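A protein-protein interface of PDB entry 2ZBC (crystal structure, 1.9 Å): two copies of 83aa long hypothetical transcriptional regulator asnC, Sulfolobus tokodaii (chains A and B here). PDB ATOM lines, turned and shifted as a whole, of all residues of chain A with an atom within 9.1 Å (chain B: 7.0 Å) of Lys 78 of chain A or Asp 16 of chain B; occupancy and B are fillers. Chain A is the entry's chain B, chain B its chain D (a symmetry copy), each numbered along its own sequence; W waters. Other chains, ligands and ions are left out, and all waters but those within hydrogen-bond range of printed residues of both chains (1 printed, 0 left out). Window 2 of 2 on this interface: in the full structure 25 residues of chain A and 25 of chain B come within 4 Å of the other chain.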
ATOM      1  N   ILE A  73     -15.648  15.108 -26.560  1.00  0.00           N
ATOM      2  CA  ILE A  73     -15.299  14.410 -25.282  1.00  0.00           C
ATOM      3  C   ILE A  73     -14.387  15.293 -24.474  1.00  0.00           C
ATOM      4  O   ILE A  73     -13.355  15.831 -24.971  1.00  0.00           O
ATOM      5  CB  ILE A  73     -14.666  13.008 -25.526  1.00  0.00           C
ATOM      6  CG1 ILE A  73     -15.576  12.138 -26.442  1.00  0.00           C
ATOM      7  CG2 ILE A  73     -14.262  12.332 -24.106  1.00  0.00           C
ATOM      8  CD1 ILE A  73     -16.969  12.042 -25.995  1.00  0.00           C
ATOM      9  N   ILE A  74     -14.818  15.628 -23.257  1.00  0.00           N
ATOM     10  CA  ILE A  74     -14.024  16.464 -22.378  1.00  0.00           C
ATOM     11  C   ILE A  74     -12.874  15.662 -21.726  1.00  0.00           C
ATOM     12  O   ILE A  74     -13.036  14.470 -21.272  1.00  0.00           O
ATOM     13  CB  ILE A  74     -14.925  17.050 -21.256  1.00  0.00           C
ATOM     14  CG1 ILE A  74     -15.837  18.075 -21.824  1.00  0.00           C
ATOM     15  CG2 ILE A  74     -14.108  17.575 -20.012  1.00  0.00           C
ATOM     16  CD1 ILE A  74     -17.038  18.342 -20.973  1.00  0.00           C
ATOM     17  N   VAL A  75     -11.709  16.273 -21.640  1.00  0.00           N
ATOM     18  CA  VAL A  75     -10.552  15.585 -21.059  1.00  0.00           C
ATOM     19  C   VAL A  75     -10.620  15.545 -19.515  1.00  0.00           C
ATOM     20  O   VAL A  75     -10.665  16.579 -18.874  1.00  0.00           O
ATOM     21  CB  VAL A  75      -9.282  16.291 -21.494  1.00  0.00           C
ATOM     22  CG1 VAL A  75      -8.119  15.755 -20.816  1.00  0.00           C
ATOM     23  CG2 VAL A  75      -9.148  16.074 -23.072  1.00  0.00           C
ATOM     24  N   GLU A  76     -10.659  14.342 -18.939  1.00  0.00           N
ATOM     25  CA  GLU A  76     -10.667  14.238 -17.493  1.00  0.00           C
ATOM     26  C   GLU A  76      -9.431  14.880 -16.938  1.00  0.00           C
ATOM     27  O   GLU A  76      -8.376  14.613 -17.399  1.00  0.00           O
ATOM     28  CB  GLU A  76     -10.669  12.730 -17.092  1.00  0.00           C
ATOM     29  CG  GLU A  76     -12.051  12.114 -17.155  1.00  0.00           C
ATOM     30  CD  GLU A  76     -12.088  10.603 -16.737  1.00  0.00           C
ATOM     31  OE1 GLU A  76     -11.057   9.946 -16.799  1.00  0.00           O
ATOM     32  OE2 GLU A  76     -13.164  10.109 -16.317  1.00  0.00           O
ATOM     33  N   GLY A  77      -9.569  15.708 -15.923  1.00  0.00           N
ATOM     34  CA  GLY A  77      -8.445  16.433 -15.365  1.00  0.00           C
ATOM     35  C   GLY A  77      -8.165  17.795 -16.019  1.00  0.00           C
ATOM     36  O   GLY A  77      -7.255  18.511 -15.582  1.00  0.00           O
ATOM     37  N   LYS A  78      -8.927  18.136 -17.052  1.00  0.00           N
ATOM     38  CA  LYS A  78      -8.771  19.425 -17.716  1.00  0.00           C
ATOM     39  C   LYS A  78     -10.166  19.991 -17.894  1.00  0.00           C
ATOM     40  O   LYS A  78     -10.572  20.387 -19.003  1.00  0.00           O
ATOM     41  CB  LYS A  78      -8.053  19.313 -19.040  1.00  0.00           C
ATOM     42  CG  LYS A  78      -6.570  18.829 -18.957  1.00  0.00           C
ATOM     43  CD  LYS A  78      -5.759  19.983 -18.308  1.00  0.00           C
ATOM     44  CE  LYS A  78      -4.320  19.653 -18.101  1.00  0.00           C
ATOM     45  NZ  LYS A  78      -4.149  18.733 -17.046  1.00  0.00           N
ATOM     46  N   SER A  79     -10.938  19.997 -16.809  1.00  0.00           N
ATOM     47  CA  SER A  79     -12.332  20.334 -16.915  1.00  0.00           C
ATOM     48  C   SER A  79     -12.727  21.046 -15.635  1.00  0.00           C
ATOM     49  O   SER A  79     -12.450  20.534 -14.553  1.00  0.00           O
ATOM     50  CB  SER A  79     -13.184  19.089 -17.151  1.00  0.00           C
ATOM     51  OG  SER A  79     -14.518  19.407 -17.186  1.00  0.00           O
ATOM     52  N   LEU A  80     -13.315  22.236 -15.743  1.00  0.00           N
ATOM     53  CA  LEU A  80     -13.786  22.916 -14.521  1.00  0.00           C
ATOM     54  C   LEU A  80     -15.077  23.621 -14.780  1.00  0.00           C
ATOM     55  O   LEU A  80     -15.183  24.366 -15.767  1.00  0.00           O
ATOM     56  CB  LEU A  80     -12.742  23.933 -14.080  1.00  0.00           C
ATOM     57  CG  LEU A  80     -13.284  24.948 -13.062  1.00  0.00           C
ATOM     58  CD1 LEU A  80     -13.530  24.223 -11.720  1.00  0.00           C
ATOM     59  CD2 LEU A  80     -12.330  26.049 -12.942  1.00  0.00           C
ATOM     60  N   VAL A  81     -16.077  23.365 -13.941  1.00  0.00           N
ATOM     61  CA  VAL A  81     -17.289  24.175 -13.867  1.00  0.00           C
ATOM     62  C   VAL A  81     -17.317  24.873 -12.494  1.00  0.00           C
ATOM     63  O   VAL A  81     -17.390  24.206 -11.478  1.00  0.00           O
ATOM     64  CB  VAL A  81     -18.594  23.298 -14.054  1.00  0.00           C
ATOM     65  CG1 VAL A  81     -19.870  24.104 -13.866  1.00  0.00           C
ATOM     66  CG2 VAL A  81     -18.615  22.619 -15.429  1.00  0.00           C
ATOM     67  N   THR B  10      -5.655  26.086 -30.257  1.00  0.00           N
ATOM     68  CA  THR B  10      -4.315  26.497 -29.816  1.00  0.00           C
ATOM     69  C   THR B  10      -3.241  26.096 -30.787  1.00  0.00           C
ATOM     70  O   THR B  10      -3.421  25.277 -31.644  1.00  0.00           O
ATOM     71  CB  THR B  10      -3.970  25.990 -28.393  1.00  0.00           C
ATOM     72  OG1 THR B  10      -3.825  24.566 -28.400  1.00  0.00           O
ATOM     73  CG2 THR B  10      -5.056  26.292 -27.410  1.00  0.00           C
ATOM     74  N   GLY B  13       0.209  21.600 -29.014  1.00  0.00           N
ATOM     75  CA  GLY B  13       0.890  21.371 -27.758  1.00  0.00           C
ATOM     76  C   GLY B  13       0.595  22.419 -26.695  1.00  0.00           C
ATOM     77  O   GLY B  13       1.027  22.251 -25.583  1.00  0.00           O
ATOM     78  N   GLY B  14      -0.102  23.513 -27.019  1.00  0.00           N
ATOM     79  CA  GLY B  14      -0.334  24.607 -26.041  1.00  0.00           C
ATOM     80  C   GLY B  14      -1.627  24.559 -25.267  1.00  0.00           C
ATOM     81  O   GLY B  14      -1.916  25.447 -24.486  1.00  0.00           O
ATOM     82  N   GLU B  15      -2.403  23.519 -25.483  1.00  0.00           N
ATOM     83  CA  GLU B  15      -3.781  23.532 -25.003  1.00  0.00           C
ATOM     84  C   GLU B  15      -3.800  23.480 -23.448  1.00  0.00           C
ATOM     85  O   GLU B  15      -4.654  24.117 -22.875  1.00  0.00           O
ATOM     86  CB  GLU B  15      -4.647  22.422 -25.594  1.00  0.00           C
ATOM     87  CG  GLU B  15      -4.111  20.953 -25.476  1.00  0.00           C
ATOM     88  CD  GLU B  15      -3.144  20.522 -26.581  1.00  0.00           C
ATOM     89  OE1 GLU B  15      -2.596  21.369 -27.312  1.00  0.00           O
ATOM     90  OE2 GLU B  15      -2.861  19.346 -26.664  1.00  0.00           O
ATOM     91  N   ASP B  16      -2.904  22.716 -22.805  1.00  0.00           N
ATOM     92  CA  ASP B  16      -2.911  22.711 -21.285  1.00  0.00           C
ATOM     93  C   ASP B  16      -2.564  24.052 -20.700  1.00  0.00           C
ATOM     94  O   ASP B  16      -3.189  24.530 -19.733  1.00  0.00           O
ATOM     95  CB  ASP B  16      -1.966  21.655 -20.731  1.00  0.00           C
ATOM     96  CG  ASP B  16      -2.410  20.280 -21.078  1.00  0.00           C
ATOM     97  OD1 ASP B  16      -3.533  20.101 -21.610  1.00  0.00           O
ATOM     98  OD2 ASP B  16      -1.706  19.306 -20.910  1.00  0.00           O
ATOM     99  N   GLU B  17      -1.571  24.702 -21.313  1.00  0.00           N
ATOM    100  CA  GLU B  17      -1.167  26.036 -20.877  1.00  0.00           C
ATOM    101  C   GLU B  17      -2.278  27.071 -21.001  1.00  0.00           C
ATOM    102  O   GLU B  17      -2.488  27.874 -20.116  1.00  0.00           O
ATOM    103  CB  GLU B  17       0.060  26.462 -21.703  1.00  0.00           C
ATOM    104  CG  GLU B  17       0.785  27.741 -21.275  1.00  0.00           C
ATOM    105  CD  GLU B  17       1.911  28.127 -22.263  1.00  0.00           C
ATOM    106  OE1 GLU B  17       2.859  27.256 -22.471  1.00  0.00           O
ATOM    107  OE2 GLU B  17       1.795  29.227 -22.860  1.00  0.00           O
ATOM    108  N   VAL B  18      -2.953  27.097 -22.125  1.00  0.00           N
ATOM    109  CA  VAL B  18      -4.032  28.046 -22.336  1.00  0.00           C
ATOM    110  C   VAL B  18      -5.161  27.725 -21.377  1.00  0.00           C
ATOM    111  O   VAL B  18      -5.710  28.624 -20.735  1.00  0.00           O
ATOM    112  CB  VAL B  18      -4.439  28.030 -23.810  1.00  0.00           C
ATOM    113  CG1 VAL B  18      -5.723  28.863 -24.160  1.00  0.00           C
ATOM    114  CG2 VAL B  18      -3.227  28.514 -24.650  1.00  0.00           C
ATOM    115  N   PHE B  19      -5.475  26.436 -21.250  1.00  0.00           N
ATOM    116  CA  PHE B  19      -6.490  26.012 -20.284  1.00  0.00           C
ATOM    117  C   PHE B  19      -6.231  26.570 -18.873  1.00  0.00           C
ATOM    118  O   PHE B  19      -7.126  27.225 -18.281  1.00  0.00           O
ATOM    119  CB  PHE B  19      -6.503  24.505 -20.186  1.00  0.00           C
ATOM    120  CG  PHE B  19      -7.309  23.997 -19.053  1.00  0.00           C
ATOM    121  CD1 PHE B  19      -8.652  23.831 -19.190  1.00  0.00           C
ATOM    122  CD2 PHE B  19      -6.673  23.545 -17.889  1.00  0.00           C
ATOM    123  CE1 PHE B  19      -9.393  23.291 -18.106  1.00  0.00           C
ATOM    124  CE2 PHE B  19      -7.419  23.034 -16.796  1.00  0.00           C
ATOM    125  CZ  PHE B  19      -8.744  22.914 -16.925  1.00  0.00           C
ATOM    126  N   GLU B  20      -4.986  26.412 -18.401  1.00  0.00           N
ATOM    127  CA  GLU B  20      -4.557  26.971 -17.108  1.00  0.00           C
ATOM    128  C   GLU B  20      -4.723  28.540 -16.982  1.00  0.00           C
ATOM    129  O   GLU B  20      -5.181  29.070 -15.959  1.00  0.00           O
ATOM    130  CB  GLU B  20      -3.142  26.499 -16.705  1.00  0.00           C
ATOM    131  CG  GLU B  20      -2.900  24.983 -16.614  1.00  0.00           C
ATOM    132  CD  GLU B  20      -3.611  24.309 -15.422  1.00  0.00           C
ATOM    133  OE1 GLU B  20      -4.235  24.993 -14.595  1.00  0.00           O
ATOM    134  OE2 GLU B  20      -3.575  23.085 -15.345  1.00  0.00           O
ATOM    135  N   ARG B  21      -4.348  29.282 -18.000  1.00  0.00           N
ATOM    136  CA  ARG B  21      -4.535  30.715 -17.979  1.00  0.00           C
ATOM    137  C   ARG B  21      -6.050  31.051 -17.892  1.00  0.00           C
ATOM    138  O   ARG B  21      -6.488  31.959 -17.151  1.00  0.00           O
ATOM    139  CB  ARG B  21      -3.888  31.314 -19.267  1.00  0.00           C
ATOM    140  CG  ARG B  21      -2.396  31.380 -19.295  1.00  0.00           C
ATOM    141  CD  ARG B  21      -1.810  32.308 -18.206  1.00  0.00           C
ATOM    142  NE  ARG B  21      -2.270  33.696 -18.281  1.00  0.00           N
ATOM    143  CZ  ARG B  21      -1.794  34.635 -19.111  1.00  0.00           C
ATOM    144  NH1 ARG B  21      -0.858  34.350 -19.952  1.00  0.00           N
ATOM    145  NH2 ARG B  21      -2.297  35.859 -19.074  1.00  0.00           N
ATOM    146  N   LEU B  22      -6.878  30.332 -18.651  1.00  0.00           N
ATOM    147  CA  LEU B  22      -8.310  30.604 -18.683  1.00  0.00           C
ATOM    148  C   LEU B  22      -9.068  30.351 -17.384  1.00  0.00           C
ATOM    149  O   LEU B  22      -9.956  31.157 -16.987  1.00  0.00           O
ATOM    150  CB  LEU B  22      -9.011  29.848 -19.829  1.00  0.00           C
ATOM    151  CG  LEU B  22      -8.571  30.389 -21.230  1.00  0.00           C
ATOM    152  CD1 LEU B  22      -8.895  29.358 -22.251  1.00  0.00           C
ATOM    153  CD2 LEU B  22      -9.359  31.605 -21.635  1.00  0.00           C
ATOM    154  N   LYS B  23      -8.713  29.226 -16.758  1.00  0.00           N
ATOM    155  CA  LYS B  23      -9.336  28.741 -15.536  1.00  0.00           C
ATOM    156  C   LYS B  23      -9.424  29.778 -14.429  1.00  0.00           C
ATOM    157  O   LYS B  23     -10.468  29.962 -13.844  1.00  0.00           O
ATOM    158  CB  LYS B  23      -8.524  27.550 -14.997  1.00  0.00           C
ATOM    159  CG  LYS B  23      -9.405  26.533 -14.434  1.00  0.00           C
ATOM    160  CD  LYS B  23      -8.678  25.156 -14.079  1.00  0.00           C
ATOM    161  CE  LYS B  23      -7.262  25.285 -13.575  1.00  0.00           C
ATOM    162  NZ  LYS B  23      -7.223  25.228 -12.060  1.00  0.00           N
ATOM    163  N   VAL B  31     -14.528  25.845 -18.261  1.00  0.00           N
ATOM    164  CA  VAL B  31     -13.443  25.626 -19.265  1.00  0.00           C
ATOM    165  C   VAL B  31     -13.050  24.165 -19.303  1.00  0.00           C
ATOM    166  O   VAL B  31     -13.029  23.477 -18.250  1.00  0.00           O
ATOM    167  CB  VAL B  31     -12.266  26.537 -18.999  1.00  0.00           C
ATOM    168  CG1 VAL B  31     -11.620  26.334 -17.644  1.00  0.00           C
ATOM    169  CG2 VAL B  31     -11.230  26.507 -20.079  1.00  0.00           C
ATOM    170  N   HIS B  32     -12.817  23.644 -20.521  1.00  0.00           N
ATOM    171  CA  HIS B  32     -12.595  22.220 -20.761  1.00  0.00           C
ATOM    172  C   HIS B  32     -11.663  22.066 -21.949  1.00  0.00           C
ATOM    173  O   HIS B  32     -11.881  22.734 -22.944  1.00  0.00           O
ATOM    174  CB  HIS B  32     -13.887  21.500 -21.135  1.00  0.00           C
ATOM    175  CG  HIS B  32     -15.068  21.808 -20.276  1.00  0.00           C
ATOM    176  ND1 HIS B  32     -15.225  21.248 -19.033  1.00  0.00           N
ATOM    177  CD2 HIS B  32     -16.204  22.516 -20.513  1.00  0.00           C
ATOM    178  CE1 HIS B  32     -16.348  21.681 -18.499  1.00  0.00           C
ATOM    179  NE2 HIS B  32     -16.957  22.460 -19.366  1.00  0.00           N
ATOM    180  N   VAL B  33     -10.626  21.254 -21.845  1.00  0.00           N
ATOM    181  CA  VAL B  33      -9.913  20.792 -23.015  1.00  0.00           C
ATOM    182  C   VAL B  33     -10.737  19.651 -23.597  1.00  0.00           C
ATOM    183  O   VAL B  33     -11.329  18.810 -22.886  1.00  0.00           O
ATOM    184  CB  VAL B  33      -8.512  20.311 -22.703  1.00  0.00           C
ATOM    185  CG1 VAL B  33      -7.827  19.700 -23.841  1.00  0.00           C
ATOM    186  CG2 VAL B  33      -7.670  21.457 -22.129  1.00  0.00           C
ATOM    187  N   VAL B  34     -10.732  19.607 -24.897  1.00  0.00           N
ATOM    188  CA  VAL B  34     -11.575  18.631 -25.618  1.00  0.00           C
ATOM    189  C   VAL B  34     -10.876  18.005 -26.775  1.00  0.00           C
ATOM    190  O   VAL B  34     -10.003  18.595 -27.411  1.00  0.00           O
ATOM    191  CB  VAL B  34     -12.884  19.228 -26.123  1.00  0.00           C
ATOM    192  CG1 VAL B  34     -13.797  19.606 -25.046  1.00  0.00           C
ATOM    193  CG2 VAL B  34     -12.607  20.492 -26.975  1.00  0.00           C
ATOM    194  N   ILE B  40     -10.334  23.764 -26.918  1.00  0.00           N
ATOM    195  CA  ILE B  40     -10.803  24.248 -25.631  1.00  0.00           C
ATOM    196  C   ILE B  40     -12.187  24.860 -25.813  1.00  0.00           C
ATOM    197  O   ILE B  40     -12.444  25.668 -26.774  1.00  0.00           O
ATOM    198  CB  ILE B  40      -9.811  25.234 -25.016  1.00  0.00           C
ATOM    199  CG1 ILE B  40      -8.462  24.627 -24.717  1.00  0.00           C
ATOM    200  CG2 ILE B  40     -10.324  25.827 -23.691  1.00  0.00           C
ATOM    201  CD1 ILE B  40      -7.439  25.676 -24.386  1.00  0.00           C
HETATM  202  O   HOH W   1      -4.864  20.881 -14.679  1.00  0.00           O
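N of Val 75 of chain A lies within hydrogen-bond range of O of Val 33 of chain B (2.9 Å).
The backbone carbonyl oxygen (O) of Lys 78 of chain A is in hydrogen-bond range of the backbone NH (N) of Val 33 of chain B.
A ring nitrogen (ND1) of His 32 of chain B lies within hydrogen-bond range of the side-chain hydroxyl (OG) of Ser 79 of chain A, at 2.7 Å.
N of Leu 80 of chain A sits at hydrogen-bond distance from O of Val 31 of chain B (2.8 Å).
The side-chain carboxylate of Glu 20 of chain B lies within salt-bridge range of the side-chain amino group of Lys 23 of chain B, at 3.9 Å.
Val 34 of chain B touches Ile 73 of chain A (CA to O, 3.4 Å).
His 32 of chain B touches Ile 74 of chain A.
Ile 74 of chain A touches Val 33 of chain B (CA to O, 3.6 Å).
Lys 78 of chain A touches Asp 16 of chain B.
Lys 78 of chain A touches Phe 19 of chain B.
O of Lys 78 of chain A touches CA of His 32 of chain B, 3.2 Å away.
Val 31 of chain B touches Ser 79 of chain A (O to CA, 3.5 Å).
Leu 80 of chain A touches Lys 23 of chain B (CD2 to CG, 3.3 Å).
ND1 of His 32 of chain B touches N of Leu 80 of chain A, 3.9 Å away.
CE1 of His 32 of chain B touches CG2 of Val 81 of chain A (3.9 Å).
Asp 16 of chain B touches just one residue of chain A: Lys 78.
No residue of chain B comes within 4 Å of Gly 77 of chain A.
Phe 19 of chain B touches two residues of chain A.
Of the printed residues of chain A, Val 33 of chain B touches Ile 74, Val 75 and Lys 78.
Printed residues of chain A within 4 Å of His 32 of chain B: Ile 74, Lys 78, Ser 79, Leu 80 and Val 81.
Printed residues of chain B within 4 Å of Ile 74 of chain A: His 32 and Val 33.
Of the printed residues of chain B, Ile 73 of chain A touches Val 34.
Of the printed residues of chain A, Lys 23 of chain B touches Leu 80 (3.3 Å).
Arg 21 of chain B touches none of the printed residues of chain A.
Val 18 of chain B touches none of the printed residues of chain A.
The nearest residue of chain A that does not touch Asp 16 of chain B is Val 75 of chain A (6.4 Å).
Of the 9 printed residues of chain A, 7 touch a printed residue of chain B.
Hydrophobic or aromatic side chains of chain B that line the printed part of chain A: Phe 19, His 32, Val 33 and Val 34.
Among the printed residues, no Asp or Glu carboxylate lies within 4 Å of a Lys or Arg side-chain nitrogen of the other chain.
No position is printed for both chains.
Of the 15 pairs that touch across the chains among the printed residues, none has its exchanged pair printed and touching as well.
Water W1 lies within hydrogen-bond range of OE2 of Glu 20 of chain B, NZ of Lys 78 of chain A and O of Gly 77 of chain A.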
